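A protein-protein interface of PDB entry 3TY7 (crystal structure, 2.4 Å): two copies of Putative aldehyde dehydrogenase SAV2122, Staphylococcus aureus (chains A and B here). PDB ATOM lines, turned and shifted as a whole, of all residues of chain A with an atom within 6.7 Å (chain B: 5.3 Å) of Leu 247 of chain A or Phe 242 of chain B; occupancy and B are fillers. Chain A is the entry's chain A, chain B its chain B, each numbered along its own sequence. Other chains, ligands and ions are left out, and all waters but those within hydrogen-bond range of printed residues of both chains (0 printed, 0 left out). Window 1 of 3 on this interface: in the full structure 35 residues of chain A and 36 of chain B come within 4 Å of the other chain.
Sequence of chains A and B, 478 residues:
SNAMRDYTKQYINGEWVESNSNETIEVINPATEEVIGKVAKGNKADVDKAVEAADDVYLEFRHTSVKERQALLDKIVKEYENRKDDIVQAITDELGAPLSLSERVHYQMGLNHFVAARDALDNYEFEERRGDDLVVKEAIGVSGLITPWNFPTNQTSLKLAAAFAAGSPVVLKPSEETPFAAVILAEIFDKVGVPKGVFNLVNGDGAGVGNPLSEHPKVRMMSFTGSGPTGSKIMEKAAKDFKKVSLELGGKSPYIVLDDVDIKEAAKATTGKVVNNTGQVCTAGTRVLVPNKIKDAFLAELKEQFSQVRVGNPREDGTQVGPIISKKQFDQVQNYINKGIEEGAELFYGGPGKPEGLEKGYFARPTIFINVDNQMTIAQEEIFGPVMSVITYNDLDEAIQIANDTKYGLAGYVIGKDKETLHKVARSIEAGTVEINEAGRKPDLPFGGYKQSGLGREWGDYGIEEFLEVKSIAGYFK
O of Ala 239 of chain B lies within hydrogen-bond range of OG of Ser 232 of chain A (2.7 Å).
The backbone carbonyl oxygen of Ala 238 of chain B lies within hydrogen-bond range of the backbone NH of Lys 243 of chain B (3.2 Å).
The side-chain amino group of Lys 243 of chain B lies within salt-bridge range of the side-chain carboxylate of Asp 241 of chain B, 3.2 Å away.
Gly 228 of chain A touches Phe 242 of chain B (O to CZ, 3.4 Å).
CE1 of Phe 242 of chain B touches OG of Ser 232 of chain A, 3.3 Å away.
Met 235 of chain A touches Ala 239 of chain B (SD to CA, 3.9 Å).
CE of Met 235 of chain A touches O of Lys 243 of chain B, at 3.98 Å.
Leu 247 of chain A touches Phe 242 of chain B (CD2 to O, 3.9 Å).
Of chain B, only Phe 242 (3.9 Å) comes within 4 Å of Leu 247 of chain A.
Of the printed residues of chain B, Met 235 of chain A touches Ala 239 and Lys 243.
Of the printed residues of chain B, Gly 228 of chain A touches Phe 242 (3.4 Å).
Phe 224 of chain A touches none of the printed residues of chain B.
The nearest printed residue of chain B that does not touch Leu 247 of chain A is Lys 243 of chain B (5.3 Å).
The nearest printed residue of chain A that does not touch Ala 239 of chain B is Gly 231 of chain A (5.5 Å).
Printed residues of chain B that touch a printed residue of chain A: Ala 239, Phe 242 and Lys 243.
Hydrophobic or aromatic side chains of chain B within 4 Å of the printed part of chain A: Phe 242.
Along chain B the printed residues that touch a printed residue of chain A span positions 239 to 243.
Of the 16 printed residues of chain A, 4 touch a printed residue of chain B.
Hydrophobic or aromatic side chains of chain A that line the printed part of chain B: Met 235 and Leu 247.
Among the printed residues, no Asp or Glu carboxylate lies within 4 Å of a Lys or Arg side-chain nitrogen of the other chain.
No position is printed for both chains.
Of the 6 pairs that touch across the chains among the printed residues, none has its exchanged pair printed and touching as well.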
ATOM      1  N   MET A 222      24.501  18.354  -0.361  1.00  0.00           N
ATOM      2  CA  MET A 222      24.079  18.398   1.031  1.00  0.00           C
ATOM      3  C   MET A 222      23.521  17.045   1.465  1.00  0.00           C
ATOM      4  O   MET A 222      22.557  16.546   0.883  1.00  0.00           O
ATOM      5  CB  MET A 222      23.029  19.496   1.226  1.00  0.00           C
ATOM      6  CG  MET A 222      22.935  20.024   2.643  1.00  0.00           C
ATOM      7  SD  MET A 222      24.489  21.090   3.145  1.00  0.00           S
ATOM      8  CE  MET A 222      24.249  21.023   5.073  1.00  0.00           C
ATOM      9  N   SER A 223      24.134  16.447   2.482  1.00  0.00           N
ATOM     10  CA  SER A 223      23.651  15.179   3.017  1.00  0.00           C
ATOM     11  C   SER A 223      23.211  15.332   4.469  1.00  0.00           C
ATOM     12  O   SER A 223      24.033  15.562   5.357  1.00  0.00           O
ATOM     13  CB  SER A 223      24.726  14.101   2.898  1.00  0.00           C
ATOM     14  OG  SER A 223      24.295  12.887   3.487  1.00  0.00           O
ATOM     15  N   PHE A 224      21.910  15.194   4.701  1.00  0.00           N
ATOM     16  CA  PHE A 224      21.336  15.418   6.023  1.00  0.00           C
ATOM     17  C   PHE A 224      20.689  14.167   6.599  1.00  0.00           C
ATOM     18  O   PHE A 224      20.121  13.352   5.873  1.00  0.00           O
ATOM     19  CB  PHE A 224      20.312  16.558   5.984  1.00  0.00           C
ATOM     20  CG  PHE A 224      19.480  16.663   7.232  1.00  0.00           C
ATOM     21  CD1 PHE A 224      20.002  17.232   8.382  1.00  0.00           C
ATOM     22  CD2 PHE A 224      18.180  16.183   7.260  1.00  0.00           C
ATOM     23  CE1 PHE A 224      19.243  17.325   9.535  1.00  0.00           C
ATOM     24  CE2 PHE A 224      17.416  16.272   8.411  1.00  0.00           C
ATOM     25  CZ  PHE A 224      17.948  16.846   9.549  1.00  0.00           C
ATOM     26  N   THR A 225      20.791  14.026   7.917  1.00  0.00           N
ATOM     27  CA  THR A 225      20.133  12.945   8.636  1.00  0.00           C
ATOM     28  C   THR A 225      19.553  13.480   9.943  1.00  0.00           C
ATOM     29  O   THR A 225      20.259  14.120  10.724  1.00  0.00           O
ATOM     30  CB  THR A 225      21.112  11.799   8.925  1.00  0.00           C
ATOM     31  OG1 THR A 225      21.793  11.437   7.718  1.00  0.00           O
ATOM     32  CG2 THR A 225      20.377  10.588   9.478  1.00  0.00           C
ATOM     33  N   SER A 227      15.569  14.854  12.020  1.00  0.00           N
ATOM     34  CA  SER A 227      14.129  15.062  12.145  1.00  0.00           C
ATOM     35  C   SER A 227      13.475  15.579  10.865  1.00  0.00           C
ATOM     36  O   SER A 227      14.142  16.121   9.984  1.00  0.00           O
ATOM     37  CB  SER A 227      13.836  16.032  13.292  1.00  0.00           C
ATOM     38  OG  SER A 227      14.379  17.314  13.023  1.00  0.00           O
ATOM     39  N   GLY A 228      12.163  15.391  10.778  1.00  0.00           N
ATOM     40  CA  GLY A 228      11.375  15.854   9.649  1.00  0.00           C
ATOM     41  C   GLY A 228      11.403  17.349   9.363  1.00  0.00           C
ATOM     42  O   GLY A 228      11.719  17.747   8.241  1.00  0.00           O
ATOM     43  N   PRO A 229      11.062  18.186  10.362  1.00  0.00           N
ATOM     44  CA  PRO A 229      11.049  19.641  10.152  1.00  0.00           C
ATOM     45  C   PRO A 229      12.396  20.212   9.709  1.00  0.00           C
ATOM     46  O   PRO A 229      12.433  21.035   8.794  1.00  0.00           O
ATOM     47  CB  PRO A 229      10.677  20.185  11.533  1.00  0.00           C
ATOM     48  CG  PRO A 229       9.872  19.104  12.149  1.00  0.00           C
ATOM     49  CD  PRO A 229      10.498  17.823  11.675  1.00  0.00           C
ATOM     50  N   THR A 230      13.480  19.783  10.348  1.00  0.00           N
ATOM     51  CA  THR A 230      14.818  20.236   9.975  1.00  0.00           C
ATOM     52  C   THR A 230      15.171  19.724   8.579  1.00  0.00           C
ATOM     53  O   THR A 230      15.876  20.390   7.819  1.00  0.00           O
ATOM     54  CB  THR A 230      15.881  19.784  11.003  1.00  0.00           C
ATOM     55  OG1 THR A 230      15.593  20.372  12.278  1.00  0.00           O
ATOM     56  CG2 THR A 230      17.277  20.209  10.569  1.00  0.00           C
ATOM     57  N   GLY A 231      14.657  18.543   8.247  1.00  0.00           N
ATOM     58  CA  GLY A 231      14.802  17.990   6.911  1.00  0.00           C
ATOM     59  C   GLY A 231      14.241  18.928   5.860  1.00  0.00           C
ATOM     60  O   GLY A 231      14.724  18.967   4.731  1.00  0.00           O
ATOM     61  N   SER A 232      13.217  19.687   6.242  1.00  0.00           N
ATOM     62  CA  SER A 232      12.632  20.697   5.370  1.00  0.00           C
ATOM     63  C   SER A 232      13.209  22.074   5.686  1.00  0.00           C
ATOM     64  O   SER A 232      14.072  22.578   4.967  1.00  0.00           O
ATOM     65  CB  SER A 232      11.110  20.721   5.526  1.00  0.00           C
ATOM     66  OG  SER A 232      10.543  19.452   5.248  1.00  0.00           O
ATOM     67  N   MET A 235      16.079  21.229   3.133  1.00  0.00           N
ATOM     68  CA  MET A 235      15.727  20.914   1.753  1.00  0.00           C
ATOM     69  C   MET A 235      15.178  22.147   1.042  1.00  0.00           C
ATOM     70  O   MET A 235      15.255  22.256  -0.182  1.00  0.00           O
ATOM     71  CB  MET A 235      14.703  19.778   1.710  1.00  0.00           C
ATOM     72  CG  MET A 235      14.504  19.158   0.336  1.00  0.00           C
ATOM     73  SD  MET A 235      13.250  17.663   0.365  1.00  0.00           S
ATOM     74  CE  MET A 235      13.372  17.125  -1.505  1.00  0.00           C
ATOM     75  N   VAL A 245      20.344  16.866  -2.649  1.00  0.00           N
ATOM     76  CA  VAL A 245      19.945  16.591  -1.271  1.00  0.00           C
ATOM     77  C   VAL A 245      19.642  15.115  -1.027  1.00  0.00           C
ATOM     78  O   VAL A 245      18.859  14.503  -1.753  1.00  0.00           O
ATOM     79  CB  VAL A 245      18.714  17.437  -0.864  1.00  0.00           C
ATOM     80  CG1 VAL A 245      18.106  16.927   0.437  1.00  0.00           C
ATOM     81  CG2 VAL A 245      19.093  18.900  -0.743  1.00  0.00           C
ATOM     82  N   SER A 246      20.269  14.551   0.003  1.00  0.00           N
ATOM     83  CA  SER A 246      19.983  13.185   0.423  1.00  0.00           C
ATOM     84  C   SER A 246      19.084  13.193   1.649  1.00  0.00           C
ATOM     85  O   SER A 246      19.505  13.586   2.739  1.00  0.00           O
ATOM     86  CB  SER A 246      21.276  12.430   0.731  1.00  0.00           C
ATOM     87  OG  SER A 246      22.001  12.160  -0.454  1.00  0.00           O
ATOM     88  N   LEU A 247      17.843  12.752   1.466  1.00  0.00           N
ATOM     89  CA  LEU A 247      16.875  12.746   2.553  1.00  0.00           C
ATOM     90  C   LEU A 247      17.121  11.618   3.552  1.00  0.00           C
ATOM     91  O   LEU A 247      17.548  10.523   3.186  1.00  0.00           O
ATOM     92  CB  LEU A 247      15.439  12.682   2.007  1.00  0.00           C
ATOM     93  CG  LEU A 247      15.105  11.895   0.730  1.00  0.00           C
ATOM     94  CD1 LEU A 247      15.502  10.424   0.812  1.00  0.00           C
ATOM     95  CD2 LEU A 247      13.620  12.020   0.418  1.00  0.00           C
ATOM     96  N   GLU A 248      16.862  11.904   4.822  1.00  0.00           N
ATOM     97  CA  GLU A 248      16.821  10.865   5.841  1.00  0.00           C
ATOM     98  C   GLU A 248      15.579  11.039   6.699  1.00  0.00           C
ATOM     99  O   GLU A 248      15.271  12.136   7.168  1.00  0.00           O
ATOM    100  CB  GLU A 248      18.095  10.845   6.681  1.00  0.00           C
ATOM    101  CG  GLU A 248      19.021   9.691   6.334  1.00  0.00           C
ATOM    102  CD  GLU A 248      18.407   8.342   6.656  1.00  0.00           C
ATOM    103  OE1 GLU A 248      17.581   8.273   7.591  1.00  0.00           O
ATOM    104  OE2 GLU A 248      18.747   7.352   5.973  1.00  0.00           O
ATOM    105  N   LEU A 249      14.872   9.936   6.896  1.00  0.00           N
ATOM    106  CA  LEU A 249      13.491   9.983   7.333  1.00  0.00           C
ATOM    107  C   LEU A 249      13.290   9.325   8.689  1.00  0.00           C
ATOM    108  O   LEU A 249      13.978   8.364   9.032  1.00  0.00           O
ATOM    109  CB  LEU A 249      12.601   9.289   6.293  1.00  0.00           C
ATOM    110  CG  LEU A 249      13.099   9.218   4.841  1.00  0.00           C
ATOM    111  CD1 LEU A 249      14.024   8.020   4.589  1.00  0.00           C
ATOM    112  CD2 LEU A 249      11.926   9.194   3.874  1.00  0.00           C
ATOM    113  N   ALA B 238       7.824  20.843  -2.653  1.00  0.00           N
ATOM    114  CA  ALA B 238       7.894  19.393  -2.515  1.00  0.00           C
ATOM    115  C   ALA B 238       8.678  18.981  -1.271  1.00  0.00           C
ATOM    116  O   ALA B 238       8.878  17.793  -1.019  1.00  0.00           O
ATOM    117  CB  ALA B 238       8.509  18.775  -3.762  1.00  0.00           C
ATOM    118  N   ALA B 239       9.118  19.967  -0.496  1.00  0.00           N
ATOM    119  CA  ALA B 239       9.931  19.705   0.687  1.00  0.00           C
ATOM    120  C   ALA B 239       9.095  19.249   1.883  1.00  0.00           C
ATOM    121  O   ALA B 239       9.615  18.634   2.814  1.00  0.00           O
ATOM    122  CB  ALA B 239      10.750  20.936   1.049  1.00  0.00           C
ATOM    123  N   LYS B 240       7.802  19.550   1.852  1.00  0.00           N
ATOM    124  CA  LYS B 240       6.904  19.167   2.936  1.00  0.00           C
ATOM    125  C   LYS B 240       6.533  17.691   2.847  1.00  0.00           C
ATOM    126  O   LYS B 240       6.448  16.994   3.860  1.00  0.00           O
ATOM    127  CB  LYS B 240       5.641  20.032   2.915  1.00  0.00           C
ATOM    128  CG  LYS B 240       4.566  19.595   3.900  1.00  0.00           C
ATOM    129  CD  LYS B 240       3.370  20.533   3.869  1.00  0.00           C
ATOM    130  CE  LYS B 240       2.225  19.999   4.712  1.00  0.00           C
ATOM    131  NZ  LYS B 240       1.062  20.930   4.720  1.00  0.00           N
ATOM    132  N   ASP B 241       6.314  17.221   1.625  1.00  0.00           N
ATOM    133  CA  ASP B 241       5.922  15.838   1.393  1.00  0.00           C
ATOM    134  C   ASP B 241       7.145  14.950   1.186  1.00  0.00           C
ATOM    135  O   ASP B 241       7.029  13.724   1.138  1.00  0.00           O
ATOM    136  CB  ASP B 241       5.007  15.755   0.171  1.00  0.00           C
ATOM    137  CG  ASP B 241       4.088  14.553   0.209  1.00  0.00           C
ATOM    138  OD1 ASP B 241       3.447  14.330   1.259  1.00  0.00           O
ATOM    139  OD2 ASP B 241       4.007  13.830  -0.807  1.00  0.00           O
ATOM    140  N   PHE B 242       8.313  15.581   1.073  1.00  0.00           N
ATOM    141  CA  PHE B 242       9.561  14.891   0.750  1.00  0.00           C
ATOM    142  C   PHE B 242       9.426  14.063  -0.523  1.00  0.00           C
ATOM    143  O   PHE B 242       9.942  12.948  -0.609  1.00  0.00           O
ATOM    144  CB  PHE B 242      10.032  14.012   1.913  1.00  0.00           C
ATOM    145  CG  PHE B 242      10.083  14.727   3.229  1.00  0.00           C
ATOM    146  CD1 PHE B 242      11.116  15.602   3.518  1.00  0.00           C
ATOM    147  CD2 PHE B 242       9.097  14.524   4.178  1.00  0.00           C
ATOM    148  CE1 PHE B 242      11.164  16.263   4.732  1.00  0.00           C
ATOM    149  CE2 PHE B 242       9.137  15.179   5.393  1.00  0.00           C
ATOM    150  CZ  PHE B 242      10.173  16.050   5.670  1.00  0.00           C
ATOM    151  N   LYS B 243       8.714  14.615  -1.500  1.00  0.00           N
ATOM    152  CA  LYS B 243       8.559  13.977  -2.798  1.00  0.00           C
ATOM    153  C   LYS B 243       9.921  13.805  -3.445  1.00  0.00           C
ATOM    154  O   LYS B 243      10.805  14.647  -3.273  1.00  0.00           O
ATOM    155  CB  LYS B 243       7.695  14.841  -3.718  1.00  0.00           C
ATOM    156  CG  LYS B 243       6.267  15.057  -3.261  1.00  0.00           C
ATOM    157  CD  LYS B 243       5.593  16.082  -4.157  1.00  0.00           C
ATOM    158  CE  LYS B 243       4.083  16.044  -4.024  1.00  0.00           C
ATOM    159  NZ  LYS B 243       3.614  16.360  -2.650  1.00  0.00           N
ATOM    160  N   LYS B 244      10.096  12.718  -4.186  1.00  0.00           N
ATOM    161  CA  LYS B 244      11.282  12.577  -5.011  1.00  0.00           C
ATOM    162  C   LYS B 244      11.177  13.601  -6.133  1.00  0.00           C
ATOM    163  O   LYS B 244      10.162  13.675  -6.825  1.00  0.00           O
ATOM    164  CB  LYS B 244      11.401  11.162  -5.574  1.00  0.00           C
ATOM    165  CG  LYS B 244      12.551  10.985  -6.554  1.00  0.00           C
ATOM    166  CD  LYS B 244      12.577   9.583  -7.135  1.00  0.00           C
ATOM    167  CE  LYS B 244      13.739   9.415  -8.100  1.00  0.00           C
ATOM    168  NZ  LYS B 244      13.809   8.029  -8.639  1.00  0.00           N
